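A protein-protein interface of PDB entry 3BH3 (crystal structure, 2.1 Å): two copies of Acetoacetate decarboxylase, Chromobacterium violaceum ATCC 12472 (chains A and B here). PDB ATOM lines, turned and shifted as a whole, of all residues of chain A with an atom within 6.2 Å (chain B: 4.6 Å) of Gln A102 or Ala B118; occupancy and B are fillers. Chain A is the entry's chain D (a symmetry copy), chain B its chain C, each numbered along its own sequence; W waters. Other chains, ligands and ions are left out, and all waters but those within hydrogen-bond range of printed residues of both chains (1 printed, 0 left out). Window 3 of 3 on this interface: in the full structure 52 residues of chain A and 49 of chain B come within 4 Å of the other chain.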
ATOM      1  N   ALA A  19      -4.224  31.801 -26.427  1.00  0.00           N
ATOM      2  CA  ALA A  19      -5.311  30.855 -26.109  1.00  0.00           C
ATOM      3  C   ALA A  19      -6.587  31.128 -26.907  1.00  0.00           C
ATOM      4  O   ALA A  19      -7.442  30.249 -27.049  1.00  0.00           O
ATOM      5  CB  ALA A  19      -5.600  30.881 -24.622  1.00  0.00           C
ATOM      6  N   LEU A  99     -19.711  26.739 -20.384  1.00  0.00           N
ATOM      7  CA  LEU A  99     -19.366  26.392 -21.780  1.00  0.00           C
ATOM      8  C   LEU A  99     -18.552  25.104 -21.850  1.00  0.00           C
ATOM      9  O   LEU A  99     -17.796  24.796 -20.934  1.00  0.00           O
ATOM     10  CB  LEU A  99     -18.475  27.465 -22.433  1.00  0.00           C
ATOM     11  CG  LEU A  99     -18.563  28.978 -22.250  1.00  0.00           C
ATOM     12  CD1 LEU A  99     -17.826  29.657 -23.340  1.00  0.00           C
ATOM     13  CD2 LEU A  99     -19.989  29.515 -22.219  1.00  0.00           C
ATOM     14  N   ASP A 100     -18.660  24.396 -22.971  1.00  0.00           N
ATOM     15  CA  ASP A 100     -17.877  23.189 -23.271  1.00  0.00           C
ATOM     16  C   ASP A 100     -16.698  23.376 -24.278  1.00  0.00           C
ATOM     17  O   ASP A 100     -16.311  22.420 -24.969  1.00  0.00           O
ATOM     18  CB  ASP A 100     -18.848  22.139 -23.826  1.00  0.00           C
ATOM     19  CG  ASP A 100     -19.589  22.624 -25.094  1.00  0.00           C
ATOM     20  OD1 ASP A 100     -19.419  23.803 -25.485  1.00  0.00           O
ATOM     21  OD2 ASP A 100     -20.345  21.835 -25.703  1.00  0.00           O
ATOM     22  N   ASP A 101     -16.144  24.588 -24.396  1.00  0.00           N
ATOM     23  CA  ASP A 101     -15.060  24.877 -25.373  1.00  0.00           C
ATOM     24  C   ASP A 101     -14.130  25.886 -24.688  1.00  0.00           C
ATOM     25  O   ASP A 101     -14.609  26.877 -24.124  1.00  0.00           O
ATOM     26  CB  ASP A 101     -15.671  25.449 -26.681  1.00  0.00           C
ATOM     27  CG  ASP A 101     -14.625  25.705 -27.836  1.00  0.00           C
ATOM     28  OD1 ASP A 101     -13.439  25.291 -27.789  1.00  0.00           O
ATOM     29  OD2 ASP A 101     -15.024  26.335 -28.843  1.00  0.00           O
ATOM     30  N   GLN A 102     -12.819  25.636 -24.707  1.00  0.00           N
ATOM     31  CA  GLN A 102     -11.910  26.441 -23.891  1.00  0.00           C
ATOM     32  C   GLN A 102     -11.626  27.857 -24.439  1.00  0.00           C
ATOM     33  O   GLN A 102     -11.739  28.814 -23.684  1.00  0.00           O
ATOM     34  CB  GLN A 102     -10.632  25.668 -23.484  1.00  0.00           C
ATOM     35  CG  GLN A 102      -9.559  26.471 -22.712  1.00  0.00           C
ATOM     36  CD  GLN A 102      -9.992  26.992 -21.338  1.00  0.00           C
ATOM     37  OE1 GLN A 102     -10.978  26.540 -20.758  1.00  0.00           O
ATOM     38  NE2 GLN A 102      -9.231  27.940 -20.805  1.00  0.00           N
ATOM     39  N   PRO A 103     -11.286  28.001 -25.742  1.00  0.00           N
ATOM     40  CA  PRO A 103     -11.010  29.370 -26.189  1.00  0.00           C
ATOM     41  C   PRO A 103     -12.108  30.395 -25.843  1.00  0.00           C
ATOM     42  O   PRO A 103     -11.768  31.451 -25.289  1.00  0.00           O
ATOM     43  CB  PRO A 103     -10.804  29.217 -27.702  1.00  0.00           C
ATOM     44  CG  PRO A 103     -10.247  27.852 -27.840  1.00  0.00           C
ATOM     45  CD  PRO A 103     -11.067  27.038 -26.840  1.00  0.00           C
ATOM     46  N   PRO A 104     -13.405  30.091 -26.106  1.00  0.00           N
ATOM     47  CA  PRO A 104     -14.422  31.069 -25.674  1.00  0.00           C
ATOM     48  C   PRO A 104     -14.462  31.267 -24.167  1.00  0.00           C
ATOM     49  O   PRO A 104     -14.890  32.325 -23.694  1.00  0.00           O
ATOM     50  CB  PRO A 104     -15.736  30.427 -26.143  1.00  0.00           C
ATOM     51  CG  PRO A 104     -15.446  29.008 -26.260  1.00  0.00           C
ATOM     52  CD  PRO A 104     -14.051  28.934 -26.759  1.00  0.00           C
ATOM     53  N   LEU A 105     -14.029  30.251 -23.425  1.00  0.00           N
ATOM     54  CA  LEU A 105     -14.038  30.289 -21.982  1.00  0.00           C
ATOM     55  C   LEU A 105     -12.974  31.257 -21.486  1.00  0.00           C
ATOM     56  O   LEU A 105     -13.308  32.185 -20.776  1.00  0.00           O
ATOM     57  CB  LEU A 105     -13.880  28.879 -21.383  1.00  0.00           C
ATOM     58  CG  LEU A 105     -14.666  28.576 -20.091  1.00  0.00           C
ATOM     59  CD1 LEU A 105     -14.802  27.061 -19.832  1.00  0.00           C
ATOM     60  CD2 LEU A 105     -14.034  29.262 -18.890  1.00  0.00           C
ATOM     61  N   ALA A 106     -11.708  31.039 -21.852  1.00  0.00           N
ATOM     62  CA  ALA A 106     -10.624  31.971 -21.489  1.00  0.00           C
ATOM     63  C   ALA A 106     -10.925  33.360 -22.048  1.00  0.00           C
ATOM     64  O   ALA A 106     -10.909  34.357 -21.314  1.00  0.00           O
ATOM     65  CB  ALA A 106      -9.264  31.480 -22.000  1.00  0.00           C
ATOM     66  N   GLY A 107     -11.203  33.408 -23.348  1.00  0.00           N
ATOM     67  CA  GLY A 107     -11.594  34.644 -24.032  1.00  0.00           C
ATOM     68  C   GLY A 107     -12.661  35.376 -23.246  1.00  0.00           C
ATOM     69  O   GLY A 107     -12.450  36.497 -22.815  1.00  0.00           O
ATOM     70  N   GLU A 110     -11.113  36.617 -19.745  1.00  0.00           N
ATOM     71  CA  GLU A 110      -9.956  37.484 -19.737  1.00  0.00           C
ATOM     72  C   GLU A 110     -10.223  38.839 -20.421  1.00  0.00           C
ATOM     73  O   GLU A 110      -9.664  39.873 -20.019  1.00  0.00           O
ATOM     74  CB  GLU A 110      -8.771  36.743 -20.339  1.00  0.00           C
ATOM     75  CG  GLU A 110      -8.125  35.835 -19.302  1.00  0.00           C
ATOM     76  CD  GLU A 110      -7.319  34.679 -19.877  1.00  0.00           C
ATOM     77  OE1 GLU A 110      -6.558  34.882 -20.839  1.00  0.00           O
ATOM     78  OE2 GLU A 110      -7.417  33.564 -19.320  1.00  0.00           O
ATOM     79  N   PHE B  98      -0.871  22.263 -20.751  1.00  0.00           N
ATOM     80  CA  PHE B  98      -2.170  21.732 -21.177  1.00  0.00           C
ATOM     81  C   PHE B  98      -2.752  20.962 -20.017  1.00  0.00           C
ATOM     82  O   PHE B  98      -2.066  20.151 -19.417  1.00  0.00           O
ATOM     83  CB  PHE B  98      -2.005  20.849 -22.418  1.00  0.00           C
ATOM     84  CG  PHE B  98      -1.389  21.578 -23.586  1.00  0.00           C
ATOM     85  CD1 PHE B  98      -2.194  22.225 -24.515  1.00  0.00           C
ATOM     86  CD2 PHE B  98      -0.014  21.665 -23.722  1.00  0.00           C
ATOM     87  CE1 PHE B  98      -1.636  22.932 -25.566  1.00  0.00           C
ATOM     88  CE2 PHE B  98       0.562  22.387 -24.779  1.00  0.00           C
ATOM     89  CZ  PHE B  98      -0.238  23.014 -25.691  1.00  0.00           C
ATOM     90  N   LEU B  99      -4.014  21.242 -19.692  1.00  0.00           N
ATOM     91  CA  LEU B  99      -4.687  20.677 -18.516  1.00  0.00           C
ATOM     92  C   LEU B  99      -6.042  20.118 -18.896  1.00  0.00           C
ATOM     93  O   LEU B  99      -6.604  20.518 -19.905  1.00  0.00           O
ATOM     94  CB  LEU B  99      -4.909  21.776 -17.468  1.00  0.00           C
ATOM     95  CG  LEU B  99      -4.001  21.983 -16.258  1.00  0.00           C
ATOM     96  CD1 LEU B  99      -2.551  22.093 -16.631  1.00  0.00           C
ATOM     97  CD2 LEU B  99      -4.398  23.221 -15.523  1.00  0.00           C
ATOM     98  N   GLN B 102     -10.850  22.566 -15.161  1.00  0.00           N
ATOM     99  CA  GLN B 102     -11.029  24.006 -15.409  1.00  0.00           C
ATOM    100  C   GLN B 102     -10.558  24.935 -14.281  1.00  0.00           C
ATOM    101  O   GLN B 102      -9.873  25.916 -14.574  1.00  0.00           O
ATOM    102  CB  GLN B 102     -12.461  24.319 -15.842  1.00  0.00           C
ATOM    103  CG  GLN B 102     -12.754  25.785 -16.168  1.00  0.00           C
ATOM    104  CD  GLN B 102     -11.817  26.403 -17.205  1.00  0.00           C
ATOM    105  OE1 GLN B 102     -11.338  25.730 -18.122  1.00  0.00           O
ATOM    106  NE2 GLN B 102     -11.578  27.707 -17.071  1.00  0.00           N
ATOM    107  N   LEU B 105      -6.997  25.606 -14.494  1.00  0.00           N
ATOM    108  CA  LEU B 105      -6.721  26.262 -15.777  1.00  0.00           C
ATOM    109  C   LEU B 105      -7.001  27.768 -15.706  1.00  0.00           C
ATOM    110  O   LEU B 105      -6.166  28.575 -16.147  1.00  0.00           O
ATOM    111  CB  LEU B 105      -7.525  25.601 -16.913  1.00  0.00           C
ATOM    112  CG  LEU B 105      -6.985  25.570 -18.339  1.00  0.00           C
ATOM    113  CD1 LEU B 105      -7.792  24.587 -19.164  1.00  0.00           C
ATOM    114  CD2 LEU B 105      -6.980  26.964 -19.024  1.00  0.00           C
ATOM    115  N   LYS B 117      -3.591  26.006 -21.712  1.00  0.00           N
ATOM    116  CA  LYS B 117      -4.632  25.676 -22.679  1.00  0.00           C
ATOM    117  C   LYS B 117      -5.276  24.330 -22.301  1.00  0.00           C
ATOM    118  O   LYS B 117      -4.773  23.649 -21.464  1.00  0.00           O
ATOM    119  CB  LYS B 117      -4.046  25.566 -24.075  1.00  0.00           C
ATOM    120  CG  LYS B 117      -3.777  26.824 -24.766  1.00  0.00           C
ATOM    121  CD  LYS B 117      -3.117  26.617 -26.050  1.00  0.00           C
ATOM    122  CE  LYS B 117      -2.661  27.914 -26.611  1.00  0.00           C
ATOM    123  NZ  LYS B 117      -1.807  27.797 -27.753  1.00  0.00           N
ATOM    124  N   ALA B 118      -6.369  23.939 -22.924  1.00  0.00           N
ATOM    125  CA  ALA B 118      -7.001  22.664 -22.604  1.00  0.00           C
ATOM    126  C   ALA B 118      -6.448  21.486 -23.418  1.00  0.00           C
ATOM    127  O   ALA B 118      -6.095  21.642 -24.538  1.00  0.00           O
ATOM    128  CB  ALA B 118      -8.463  22.774 -22.769  1.00  0.00           C
ATOM    129  N   GLY B 119      -6.404  20.303 -22.836  1.00  0.00           N
ATOM    130  CA  GLY B 119      -5.837  19.140 -23.516  1.00  0.00           C
ATOM    131  C   GLY B 119      -6.122  17.936 -22.658  1.00  0.00           C
ATOM    132  O   GLY B 119      -6.695  18.079 -21.573  1.00  0.00           O
ATOM    133  N   PHE B 136      -4.640  16.753 -28.043  1.00  0.00           N
ATOM    134  CA  PHE B 136      -5.349  18.000 -28.179  1.00  0.00           C
ATOM    135  C   PHE B 136      -6.564  17.699 -29.073  1.00  0.00           C
ATOM    136  O   PHE B 136      -6.412  17.561 -30.291  1.00  0.00           O
ATOM    137  CB  PHE B 136      -4.431  19.070 -28.806  1.00  0.00           C
ATOM    138  CG  PHE B 136      -4.947  20.485 -28.658  1.00  0.00           C
ATOM    139  CD1 PHE B 136      -5.823  21.022 -29.603  1.00  0.00           C
ATOM    140  CD2 PHE B 136      -4.558  21.274 -27.569  1.00  0.00           C
ATOM    141  CE1 PHE B 136      -6.320  22.313 -29.475  1.00  0.00           C
ATOM    142  CE2 PHE B 136      -5.052  22.574 -27.415  1.00  0.00           C
ATOM    143  CZ  PHE B 136      -5.940  23.099 -28.373  1.00  0.00           C
HETATM  144  O   HOH W   1     -10.077  29.490 -18.673  1.00  0.00           O
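Of the 8 printed residues of chain B, 4 touch a printed residue of chain A. Hydrophobic or aromatic side chains of chain B within 4 Å of the printed part of chain A: Leu B105 and Ala B118. Among the printed residues, 5 pairs touch across the chains.
Gln B102 touches its own counterpart, Gln A102. Gln A102 touches Leu B105, and with the chains exchanged Leu A105 touches Gln B102. Positions printed for both chains: 99, 102 and 105. Of the 5 pairs that touch across the chains among the printed residues, 3 have their exchanged pair printed and touching as well.
The backbone NH of Leu B99 is in hydrogen-bond range of the backbone carbonyl oxygen of Lys B117 (3.1 Å).
Water W1 lies within hydrogen-bond range of the side-chain amide nitrogen of Gln A102 and the side-chain amide nitrogen of Gln B102.
Printed residues of chain B within 4 Å of Gln A102: Gln B102 (2.8 Å), Leu B105 (3.0 Å) and Ala B118 (3.7 Å). Ala B118 touches just one residue of chain A: Gln A102. Of the printed residues of chain A, Lys B117 touches Ala A19 (3.99 Å). Printed residues of chain A within 4 Å of Gln B102: Gln A102 (2.8 Å) and Leu A105 (3.4 Å). Of the printed residues of chain B, Ala A19 touches Lys B117. Of the printed residues of chain A, Leu B105 touches Gln A102. Of the printed residues of chain B, Leu A105 touches Gln B102. Pro A103 touches none of the printed residues of chain B. The nearest printed residue of chain B that does not touch Gln A102 is Lys B117 (4.8 Å). The nearest printed residue of chain A that does not touch Ala B118 is Pro A103 (6.4 Å). The nearest printed residue of chain B that does not touch Leu A105 is Leu B105 (7.4 Å).
OE1 of Gln B102 lies close to OE1 of Gln A102 (2.8 Å).
Ala A19 touches Lys B117 (CA to CE, 3.99 Å). NE2 of Gln A102 touches CD2 of Leu B105, at 3.0 Å. CB of Gln A102 touches CB of Ala B118 (3.7 Å). Leu A105 touches Gln B102.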
